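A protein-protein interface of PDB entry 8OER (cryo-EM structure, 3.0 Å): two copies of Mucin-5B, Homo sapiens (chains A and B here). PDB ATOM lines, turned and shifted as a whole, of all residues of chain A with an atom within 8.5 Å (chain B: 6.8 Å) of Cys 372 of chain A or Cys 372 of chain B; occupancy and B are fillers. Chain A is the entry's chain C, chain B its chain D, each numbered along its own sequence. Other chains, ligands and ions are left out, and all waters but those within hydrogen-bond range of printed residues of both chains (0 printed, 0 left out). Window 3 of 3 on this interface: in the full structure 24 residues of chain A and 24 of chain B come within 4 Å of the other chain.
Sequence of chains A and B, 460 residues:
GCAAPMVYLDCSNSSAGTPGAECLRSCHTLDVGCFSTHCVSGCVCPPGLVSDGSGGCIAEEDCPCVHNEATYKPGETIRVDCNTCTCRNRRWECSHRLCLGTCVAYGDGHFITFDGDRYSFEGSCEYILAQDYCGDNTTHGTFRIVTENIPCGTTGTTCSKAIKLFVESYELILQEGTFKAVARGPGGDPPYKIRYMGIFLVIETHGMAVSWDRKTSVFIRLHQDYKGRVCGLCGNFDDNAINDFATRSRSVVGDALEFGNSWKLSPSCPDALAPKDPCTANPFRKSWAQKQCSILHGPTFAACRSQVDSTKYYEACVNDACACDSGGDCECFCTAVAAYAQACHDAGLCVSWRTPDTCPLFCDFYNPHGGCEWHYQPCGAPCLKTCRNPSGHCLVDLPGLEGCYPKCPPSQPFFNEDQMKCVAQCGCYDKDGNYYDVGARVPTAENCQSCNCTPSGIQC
The side-chain sulfur (SG) of Cys 372 of chain A is disulfide-bonded to the side-chain sulfur (SG) of Cys 372 of chain B (2.0 Å).
OD1 of Asp 364 of chain A is in hydrogen-bond range of ND2 of Asn 367 of chain A, at 2.6 Å. The backbone carbonyl oxygen (O) of Glu 373 of chain A sits close to a ring nitrogen (NE2) of His 375 of chain A (3.5 Å). N of Tyr 405 of chain A is in hydrogen-bond range of O of His 375 of chain A. The backbone NH (N) of Trp 374 of chain B lies within hydrogen-bond range of the side-chain amide oxygen (OD1) of Asn 367 of chain B. The backbone carbonyl oxygen (O) of Cys 372 of chain B is in hydrogen-bond range of a ring nitrogen (NE2) of His 375 of chain B, at 2.7 Å. The side-chain sulfur (SG) of Cys 408 of chain A forms a disulfide with the side-chain sulfur (SG) of Cys 422 of chain A, at 2.0 Å.
Among the printed residues, merely in contact across the chains: Asp 364 of chain A with His 375 of chain B (3.2 Å), His 375 of chain A with Asp 364 of chain B (3.6 Å), Cys 372 of chain A with His 375 of chain B (3.8 Å), His 375 of chain A with Cys 372 of chain B (3.8 Å) and Asp 364 of chain A with Trp 374 of chain B (3.97 Å).
Cys 372 of chain A touches just these residues of chain B: Cys 372 (2.0 Å) and His 375 (3.8 Å). Of chain A, only Cys 372 and His 375 come within 4 Å of Cys 372 of chain B. Of the printed residues of chain A, Asp 364 of chain B touches His 375. Of the printed residues of chain B, His 375 of chain A touches Asp 364 (3.6 Å) and Cys 372 (3.8 Å). Of the printed residues of chain B, Asp 364 of chain A touches Trp 374 and His 375. Printed residues of chain A within 4 Å of Trp 374 of chain B: Asp 364. Of the printed residues of chain A, His 375 of chain B touches Asp 364 (3.2 Å) and Cys 372 (3.8 Å). Gly 370 of chain A touches none of the printed residues of chain B. The nearest residue of chain B that does not touch Cys 372 of chain A is Gly 370 of chain B (5.0 Å). The nearest printed residue of chain B that does not touch Asp 364 of chain A is Asp 364 of chain B (5.8 Å).
Hydrophobic or aromatic side chains of chain A that line the printed part of chain B: His 375. Among the printed residues, no Asp or Glu carboxylate lies within 4 Å of a Lys or Arg side-chain nitrogen of the other chain.
Asp 364 of chain A touches Trp 374 of chain B, but with the chains exchanged Trp 374 of chain A does not touch Asp 364 of chain B (5.0 Å). Asp 364 of chain A touches His 375 of chain B, and with the chains exchanged His 375 of chain A touches Asp 364 of chain B. Cys 372 of chain A touches its own counterpart, Cys 372 of chain B. Cys 372 of chain A touches His 375 of chain B, and with the chains exchanged His 375 of chain A touches Cys 372 of chain B. Positions printed for both chains: 364, 367, 368, 369, 370, 371, 372, 373, 374, 375 and 407. Of the 6 pairs that touch across the chains among the printed residues, 5 have their exchanged pair printed and touching as well.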
ATOM      1  N   CYS A 363     -18.147 -10.008   4.370  1.00  0.00           N
ATOM      2  CA  CYS A 363     -17.436  -8.756   4.540  1.00  0.00           C
ATOM      3  C   CYS A 363     -17.622  -7.819   3.365  1.00  0.00           C
ATOM      4  O   CYS A 363     -17.163  -6.675   3.423  1.00  0.00           O
ATOM      5  CB  CYS A 363     -15.951  -9.028   4.782  1.00  0.00           C
ATOM      6  SG  CYS A 363     -15.687  -9.760   6.400  1.00  0.00           S
ATOM      7  N   ASP A 364     -18.285  -8.269   2.304  1.00  0.00           N
ATOM      8  CA  ASP A 364     -18.760  -7.375   1.262  1.00  0.00           C
ATOM      9  C   ASP A 364     -19.925  -6.523   1.729  1.00  0.00           C
ATOM     10  O   ASP A 364     -20.288  -5.564   1.044  1.00  0.00           O
ATOM     11  CB  ASP A 364     -19.184  -8.190   0.044  1.00  0.00           C
ATOM     12  CG  ASP A 364     -18.560  -7.692  -1.226  1.00  0.00           C
ATOM     13  OD1 ASP A 364     -17.872  -6.652  -1.181  1.00  0.00           O
ATOM     14  OD2 ASP A 364     -18.764  -8.336  -2.274  1.00  0.00           O
ATOM     15  N   TYR A 366     -20.517  -4.340   4.202  1.00  0.00           N
ATOM     16  CA  TYR A 366     -20.266  -2.929   4.453  1.00  0.00           C
ATOM     17  C   TYR A 366     -19.642  -2.227   3.258  1.00  0.00           C
ATOM     18  O   TYR A 366     -19.346  -1.032   3.342  1.00  0.00           O
ATOM     19  CB  TYR A 366     -19.382  -2.771   5.687  1.00  0.00           C
ATOM     20  CG  TYR A 366     -19.545  -3.908   6.655  1.00  0.00           C
ATOM     21  CD1 TYR A 366     -20.724  -4.080   7.350  1.00  0.00           C
ATOM     22  CD2 TYR A 366     -18.529  -4.815   6.863  1.00  0.00           C
ATOM     23  CE1 TYR A 366     -20.884  -5.118   8.229  1.00  0.00           C
ATOM     24  CE2 TYR A 366     -18.679  -5.858   7.742  1.00  0.00           C
ATOM     25  CZ  TYR A 366     -19.859  -6.004   8.422  1.00  0.00           C
ATOM     26  OH  TYR A 366     -20.016  -7.047   9.300  1.00  0.00           O
ATOM     27  N   ASN A 367     -19.432  -2.939   2.164  1.00  0.00           N
ATOM     28  CA  ASN A 367     -19.008  -2.330   0.918  1.00  0.00           C
ATOM     29  C   ASN A 367     -20.228  -1.750   0.219  1.00  0.00           C
ATOM     30  O   ASN A 367     -21.078  -2.506  -0.265  1.00  0.00           O
ATOM     31  CB  ASN A 367     -18.324  -3.361   0.023  1.00  0.00           C
ATOM     32  CG  ASN A 367     -16.946  -3.730   0.509  1.00  0.00           C
ATOM     33  OD1 ASN A 367     -16.204  -2.883   0.992  1.00  0.00           O
ATOM     34  ND2 ASN A 367     -16.586  -4.997   0.362  1.00  0.00           N
ATOM     35  N   PRO A 368     -20.367  -0.431   0.158  1.00  0.00           N
ATOM     36  CA  PRO A 368     -21.515   0.145  -0.546  1.00  0.00           C
ATOM     37  C   PRO A 368     -21.258   0.361  -2.028  1.00  0.00           C
ATOM     38  O   PRO A 368     -20.410   1.177  -2.404  1.00  0.00           O
ATOM     39  CB  PRO A 368     -21.735   1.477   0.182  1.00  0.00           C
ATOM     40  CG  PRO A 368     -20.419   1.786   0.872  1.00  0.00           C
ATOM     41  CD  PRO A 368     -19.488   0.610   0.706  1.00  0.00           C
ATOM     42  N   HIS A 369     -21.998  -0.361  -2.867  1.00  0.00           N
ATOM     43  CA  HIS A 369     -22.090  -0.100  -4.302  1.00  0.00           C
ATOM     44  C   HIS A 369     -20.715  -0.016  -4.963  1.00  0.00           C
ATOM     45  O   HIS A 369     -20.317   1.011  -5.514  1.00  0.00           O
ATOM     46  CB  HIS A 369     -22.897   1.172  -4.560  1.00  0.00           C
ATOM     47  CG  HIS A 369     -24.324   1.075  -4.123  1.00  0.00           C
ATOM     48  ND1 HIS A 369     -25.190   2.145  -4.168  1.00  0.00           N
ATOM     49  CD2 HIS A 369     -25.035   0.034  -3.632  1.00  0.00           C
ATOM     50  CE1 HIS A 369     -26.375   1.766  -3.725  1.00  0.00           C
ATOM     51  NE2 HIS A 369     -26.308   0.490  -3.393  1.00  0.00           N
ATOM     52  N   GLY A 370     -19.986  -1.127  -4.897  1.00  0.00           N
ATOM     53  CA  GLY A 370     -18.706  -1.230  -5.560  1.00  0.00           C
ATOM     54  C   GLY A 370     -17.537  -0.630  -4.814  1.00  0.00           C
ATOM     55  O   GLY A 370     -16.400  -0.742  -5.291  1.00  0.00           O
ATOM     56  N   GLY A 371     -17.768   0.016  -3.676  1.00  0.00           N
ATOM     57  CA  GLY A 371     -16.660   0.442  -2.842  1.00  0.00           C
ATOM     58  C   GLY A 371     -15.965  -0.762  -2.237  1.00  0.00           C
ATOM     59  O   GLY A 371     -16.603  -1.701  -1.765  1.00  0.00           O
ATOM     60  N   CYS A 372     -14.639  -0.740  -2.262  1.00  0.00           N
ATOM     61  CA  CYS A 372     -13.862  -1.923  -1.909  1.00  0.00           C
ATOM     62  C   CYS A 372     -12.771  -1.571  -0.903  1.00  0.00           C
ATOM     63  O   CYS A 372     -11.604  -1.947  -1.029  1.00  0.00           O
ATOM     64  CB  CYS A 372     -13.378  -2.603  -3.195  1.00  0.00           C
ATOM     65  SG  CYS A 372     -11.748  -2.248  -3.884  1.00  0.00           S
ATOM     66  N   GLU A 373     -13.165  -0.848   0.147  1.00  0.00           N
ATOM     67  CA  GLU A 373     -12.304  -0.737   1.317  1.00  0.00           C
ATOM     68  C   GLU A 373     -12.363  -2.005   2.156  1.00  0.00           C
ATOM     69  O   GLU A 373     -11.329  -2.607   2.459  1.00  0.00           O
ATOM     70  CB  GLU A 373     -12.703   0.459   2.177  1.00  0.00           C
ATOM     71  CG  GLU A 373     -13.308   1.618   1.444  1.00  0.00           C
ATOM     72  CD  GLU A 373     -14.792   1.444   1.243  1.00  0.00           C
ATOM     73  OE1 GLU A 373     -15.182   0.572   0.441  1.00  0.00           O
ATOM     74  OE2 GLU A 373     -15.568   2.158   1.910  1.00  0.00           O
ATOM     75  N   TRP A 374     -13.566  -2.432   2.526  1.00  0.00           N
ATOM     76  CA  TRP A 374     -13.736  -3.476   3.529  1.00  0.00           C
ATOM     77  C   TRP A 374     -13.227  -4.810   3.008  1.00  0.00           C
ATOM     78  O   TRP A 374     -13.862  -5.436   2.156  1.00  0.00           O
ATOM     79  CB  TRP A 374     -15.201  -3.563   3.936  1.00  0.00           C
ATOM     80  CG  TRP A 374     -15.612  -2.377   4.720  1.00  0.00           C
ATOM     81  CD1 TRP A 374     -16.036  -1.182   4.233  1.00  0.00           C
ATOM     82  CD2 TRP A 374     -15.600  -2.250   6.143  1.00  0.00           C
ATOM     83  NE1 TRP A 374     -16.307  -0.321   5.266  1.00  0.00           N
ATOM     84  CE2 TRP A 374     -16.045  -0.956   6.449  1.00  0.00           C
ATOM     85  CE3 TRP A 374     -15.264  -3.110   7.186  1.00  0.00           C
ATOM     86  CZ2 TRP A 374     -16.161  -0.504   7.752  1.00  0.00           C
ATOM     87  CZ3 TRP A 374     -15.381  -2.659   8.476  1.00  0.00           C
ATOM     88  CH2 TRP A 374     -15.827  -1.371   8.750  1.00  0.00           C
ATOM     89  N   HIS A 375     -12.086  -5.251   3.532  1.00  0.00           N
ATOM     90  CA  HIS A 375     -11.474  -6.515   3.159  1.00  0.00           C
ATOM     91  C   HIS A 375     -11.223  -7.339   4.411  1.00  0.00           C
ATOM     92  O   HIS A 375     -10.965  -6.793   5.485  1.00  0.00           O
ATOM     93  CB  HIS A 375     -10.153  -6.303   2.416  1.00  0.00           C
ATOM     94  CG  HIS A 375     -10.280  -5.494   1.162  1.00  0.00           C
ATOM     95  ND1 HIS A 375     -11.124  -5.843   0.131  1.00  0.00           N
ATOM     96  CD2 HIS A 375      -9.655  -4.360   0.767  1.00  0.00           C
ATOM     97  CE1 HIS A 375     -11.021  -4.954  -0.840  1.00  0.00           C
ATOM     98  NE2 HIS A 375     -10.135  -4.044  -0.480  1.00  0.00           N
ATOM     99  N   TYR A 405     -11.628  -5.427   7.961  1.00  0.00           N
ATOM    100  CA  TYR A 405     -11.283  -4.058   8.268  1.00  0.00           C
ATOM    101  C   TYR A 405     -11.380  -3.227   7.006  1.00  0.00           C
ATOM    102  O   TYR A 405     -11.249  -3.751   5.898  1.00  0.00           O
ATOM    103  CB  TYR A 405      -9.861  -3.957   8.833  1.00  0.00           C
ATOM    104  CG  TYR A 405      -9.616  -4.856  10.014  1.00  0.00           C
ATOM    105  CD1 TYR A 405      -9.398  -6.209   9.841  1.00  0.00           C
ATOM    106  CD2 TYR A 405      -9.605  -4.353  11.298  1.00  0.00           C
ATOM    107  CE1 TYR A 405      -9.183  -7.029  10.904  1.00  0.00           C
ATOM    108  CE2 TYR A 405      -9.387  -5.172  12.369  1.00  0.00           C
ATOM    109  CZ  TYR A 405      -9.180  -6.509  12.162  1.00  0.00           C
ATOM    110  OH  TYR A 405      -8.955  -7.343  13.221  1.00  0.00           O
ATOM    111  N   PRO A 406     -11.629  -1.955   7.142  1.00  0.00           N
ATOM    112  CA  PRO A 406     -11.651  -1.090   5.969  1.00  0.00           C
ATOM    113  C   PRO A 406     -10.292  -0.487   5.687  1.00  0.00           C
ATOM    114  O   PRO A 406      -9.605  -0.024   6.599  1.00  0.00           O
ATOM    115  CB  PRO A 406     -12.678  -0.028   6.354  1.00  0.00           C
ATOM    116  CG  PRO A 406     -12.582   0.063   7.821  1.00  0.00           C
ATOM    117  CD  PRO A 406     -12.093  -1.255   8.347  1.00  0.00           C
ATOM    118  N   LYS A 407      -9.892  -0.501   4.418  1.00  0.00           N
ATOM    119  CA  LYS A 407      -8.660   0.145   3.982  1.00  0.00           C
ATOM    120  C   LYS A 407      -9.014   1.577   3.607  1.00  0.00           C
ATOM    121  O   LYS A 407      -9.169   1.930   2.437  1.00  0.00           O
ATOM    122  CB  LYS A 407      -8.033  -0.615   2.822  1.00  0.00           C
ATOM    123  CG  LYS A 407      -6.677  -0.097   2.390  1.00  0.00           C
ATOM    124  CD  LYS A 407      -5.621  -0.316   3.461  1.00  0.00           C
ATOM    125  CE  LYS A 407      -5.669  -1.725   4.029  1.00  0.00           C
ATOM    126  NZ  LYS A 407      -5.050  -1.786   5.382  1.00  0.00           N
ATOM    127  N   CYS A 408      -9.154   2.407   4.631  1.00  0.00           N
ATOM    128  CA  CYS A 408      -9.648   3.760   4.445  1.00  0.00           C
ATOM    129  C   CYS A 408      -8.670   4.574   3.605  1.00  0.00           C
ATOM    130  O   CYS A 408      -7.518   4.763   4.019  1.00  0.00           O
ATOM    131  CB  CYS A 408      -9.866   4.422   5.797  1.00  0.00           C
ATOM    132  SG  CYS A 408     -11.333   3.844   6.672  1.00  0.00           S
ATOM    133  N   PRO A 409      -9.083   5.080   2.448  1.00  0.00           N
ATOM    134  CA  PRO A 409      -8.157   5.779   1.568  1.00  0.00           C
ATOM    135  C   PRO A 409      -7.846   7.161   2.107  1.00  0.00           C
ATOM    136  O   PRO A 409      -8.556   7.657   2.994  1.00  0.00           O
ATOM    137  CB  PRO A 409      -8.934   5.855   0.248  1.00  0.00           C
ATOM    138  CG  PRO A 409     -10.343   5.933   0.679  1.00  0.00           C
ATOM    139  CD  PRO A 409     -10.452   5.078   1.912  1.00  0.00           C
ATOM    140  N   CYS A 422     -15.609   4.240   5.697  1.00  0.00           N
ATOM    141  CA  CYS A 422     -14.504   5.181   5.569  1.00  0.00           C
ATOM    142  C   CYS A 422     -15.049   6.501   5.046  1.00  0.00           C
ATOM    143  O   CYS A 422     -15.639   6.549   3.962  1.00  0.00           O
ATOM    144  CB  CYS A 422     -13.424   4.644   4.633  1.00  0.00           C
ATOM    145  SG  CYS A 422     -12.568   3.174   5.208  1.00  0.00           S
ATOM    146  N   ASP B 364     -15.036 -12.325  -0.255  1.00  0.00           N
ATOM    147  CA  ASP B 364     -13.685 -11.794  -0.249  1.00  0.00           C
ATOM    148  C   ASP B 364     -12.648 -12.874  -0.519  1.00  0.00           C
ATOM    149  O   ASP B 364     -11.478 -12.553  -0.741  1.00  0.00           O
ATOM    150  CB  ASP B 364     -13.424 -11.126   1.099  1.00  0.00           C
ATOM    151  CG  ASP B 364     -12.231 -10.209   1.069  1.00  0.00           C
ATOM    152  OD1 ASP B 364     -11.989  -9.580   0.012  1.00  0.00           O
ATOM    153  OD2 ASP B 364     -11.543 -10.097   2.104  1.00  0.00           O
ATOM    154  N   ASN B 367     -10.597 -12.719  -3.637  1.00  0.00           N
ATOM    155  CA  ASN B 367      -9.829 -11.495  -3.763  1.00  0.00           C
ATOM    156  C   ASN B 367      -8.367 -11.810  -3.474  1.00  0.00           C
ATOM    157  O   ASN B 367      -8.045 -12.273  -2.373  1.00  0.00           O
ATOM    158  CB  ASN B 367     -10.341 -10.433  -2.791  1.00  0.00           C
ATOM    159  CG  ASN B 367     -11.632  -9.796  -3.247  1.00  0.00           C
ATOM    160  OD1 ASN B 367     -11.831  -9.565  -4.436  1.00  0.00           O
ATOM    161  ND2 ASN B 367     -12.505  -9.481  -2.300  1.00  0.00           N
ATOM    162  N   PRO B 368      -7.460 -11.605  -4.426  1.00  0.00           N
ATOM    163  CA  PRO B 368      -6.040 -11.770  -4.127  1.00  0.00           C
ATOM    164  C   PRO B 368      -5.345 -10.530  -3.586  1.00  0.00           C
ATOM    165  O   PRO B 368      -5.066  -9.585  -4.331  1.00  0.00           O
ATOM    166  CB  PRO B 368      -5.497 -12.188  -5.502  1.00  0.00           C
ATOM    167  CG  PRO B 368      -6.632 -11.560  -6.501  1.00  0.00           C
ATOM    168  CD  PRO B 368      -7.424 -10.690  -5.570  1.00  0.00           C
ATOM    169  N   HIS B 369      -4.995 -10.568  -2.305  1.00  0.00           N
ATOM    170  CA  HIS B 369      -4.184  -9.540  -1.655  1.00  0.00           C
ATOM    171  C   HIS B 369      -4.633  -8.134  -2.054  1.00  0.00           C
ATOM    172  O   HIS B 369      -3.867  -7.331  -2.588  1.00  0.00           O
ATOM    173  CB  HIS B 369      -2.700  -9.752  -1.963  1.00  0.00           C
ATOM    174  CG  HIS B 369      -2.193 -11.107  -1.582  1.00  0.00           C
ATOM    175  ND1 HIS B 369      -0.912 -11.527  -1.865  1.00  0.00           N
ATOM    176  CD2 HIS B 369      -2.797 -12.141  -0.953  1.00  0.00           C
ATOM    177  CE1 HIS B 369      -0.746 -12.760  -1.418  1.00  0.00           C
ATOM    178  NE2 HIS B 369      -1.877 -13.156  -0.862  1.00  0.00           N
ATOM    179  N   GLY B 370      -5.907  -7.852  -1.794  1.00  0.00           N
ATOM    180  CA  GLY B 370      -6.467  -6.543  -2.047  1.00  0.00           C
ATOM    181  C   GLY B 370      -7.119  -6.359  -3.398  1.00  0.00           C
ATOM    182  O   GLY B 370      -7.911  -5.422  -3.557  1.00  0.00           O
ATOM    183  N   GLY B 371      -6.815  -7.207  -4.377  1.00  0.00           N
ATOM    184  CA  GLY B 371      -7.523  -7.142  -5.643  1.00  0.00           C
ATOM    185  C   GLY B 371      -9.006  -7.391  -5.438  1.00  0.00           C
ATOM    186  O   GLY B 371      -9.413  -8.388  -4.843  1.00  0.00           O
ATOM    187  N   CYS B 372      -9.823  -6.479  -5.949  1.00  0.00           N
ATOM    188  CA  CYS B 372     -11.217  -6.378  -5.539  1.00  0.00           C
ATOM    189  C   CYS B 372     -12.154  -6.433  -6.742  1.00  0.00           C
ATOM    190  O   CYS B 372     -13.060  -5.614  -6.906  1.00  0.00           O
ATOM    191  CB  CYS B 372     -11.395  -5.133  -4.666  1.00  0.00           C
ATOM    192  SG  CYS B 372     -11.639  -3.529  -5.457  1.00  0.00           S
ATOM    193  N   GLU B 373     -11.950  -7.424  -7.613  1.00  0.00           N
ATOM    194  CA  GLU B 373     -12.980  -7.718  -8.603  1.00  0.00           C
ATOM    195  C   GLU B 373     -14.195  -8.367  -7.954  1.00  0.00           C
ATOM    196  O   GLU B 373     -15.332  -7.952  -8.193  1.00  0.00           O
ATOM    197  CB  GLU B 373     -12.441  -8.633  -9.700  1.00  0.00           C
ATOM    198  CG  GLU B 373     -10.987  -8.477 -10.032  1.00  0.00           C
ATOM    199  CD  GLU B 373     -10.115  -9.317  -9.143  1.00  0.00           C
ATOM    200  OE1 GLU B 373     -10.037  -9.019  -7.936  1.00  0.00           O
ATOM    201  OE2 GLU B 373      -9.521 -10.287  -9.651  1.00  0.00           O
ATOM    202  N   TRP B 374     -13.967  -9.369  -7.112  1.00  0.00           N
ATOM    203  CA  TRP B 374     -15.029 -10.234  -6.608  1.00  0.00           C
ATOM    204  C   TRP B 374     -15.959  -9.463  -5.688  1.00  0.00           C
ATOM    205  O   TRP B 374     -15.617  -9.186  -4.536  1.00  0.00           O
ATOM    206  CB  TRP B 374     -14.403 -11.420  -5.891  1.00  0.00           C
ATOM    207  CG  TRP B 374     -13.718 -12.303  -6.850  1.00  0.00           C
ATOM    208  CD1 TRP B 374     -12.383 -12.394  -7.064  1.00  0.00           C
ATOM    209  CD2 TRP B 374     -14.331 -13.262  -7.711  1.00  0.00           C
ATOM    210  NE1 TRP B 374     -12.124 -13.329  -8.033  1.00  0.00           N
ATOM    211  CE2 TRP B 374     -13.308 -13.880  -8.440  1.00  0.00           C
ATOM    212  CE3 TRP B 374     -15.649 -13.651  -7.941  1.00  0.00           C
ATOM    213  CZ2 TRP B 374     -13.560 -14.864  -9.379  1.00  0.00           C
ATOM    214  CZ3 TRP B 374     -15.894 -14.629  -8.868  1.00  0.00           C
ATOM    215  CH2 TRP B 374     -14.858 -15.224  -9.577  1.00  0.00           C
ATOM    216  N   HIS B 375     -17.145  -9.133  -6.190  1.00  0.00           N
ATOM    217  CA  HIS B 375     -18.152  -8.422  -5.422  1.00  0.00           C
ATOM    218  C   HIS B 375     -19.442  -9.220  -5.431  1.00  0.00           C
ATOM    219  O   HIS B 375     -19.771  -9.888  -6.413  1.00  0.00           O
ATOM    220  CB  HIS B 375     -18.410  -7.022  -5.982  1.00  0.00           C
ATOM    221  CG  HIS B 375     -17.207  -6.134  -5.975  1.00  0.00           C
ATOM    222  ND1 HIS B 375     -16.452  -5.912  -4.845  1.00  0.00           N
ATOM    223  CD2 HIS B 375     -16.643  -5.391  -6.956  1.00  0.00           C
ATOM    224  CE1 HIS B 375     -15.466  -5.083  -5.134  1.00  0.00           C
ATOM    225  NE2 HIS B 375     -15.560  -4.750  -6.408  1.00  0.00           N
ATOM    226  N   LYS B 407     -15.832  -8.376 -11.180  1.00  0.00           N
ATOM    227  CA  LYS B 407     -15.905  -7.234 -12.083  1.00  0.00           C
ATOM    228  C   LYS B 407     -14.601  -7.206 -12.868  1.00  0.00           C
ATOM    229  O   LYS B 407     -13.714  -6.382 -12.641  1.00  0.00           O
ATOM    230  CB  LYS B 407     -16.140  -5.944 -11.308  1.00  0.00           C
ATOM    231  CG  LYS B 407     -16.419  -4.733 -12.179  1.00  0.00           C
ATOM    232  CD  LYS B 407     -17.772  -4.849 -12.863  1.00  0.00           C
ATOM    233  CE  LYS B 407     -18.859  -5.254 -11.877  1.00  0.00           C
ATOM    234  NZ  LYS B 407     -19.998  -5.933 -12.551  1.00  0.00           N
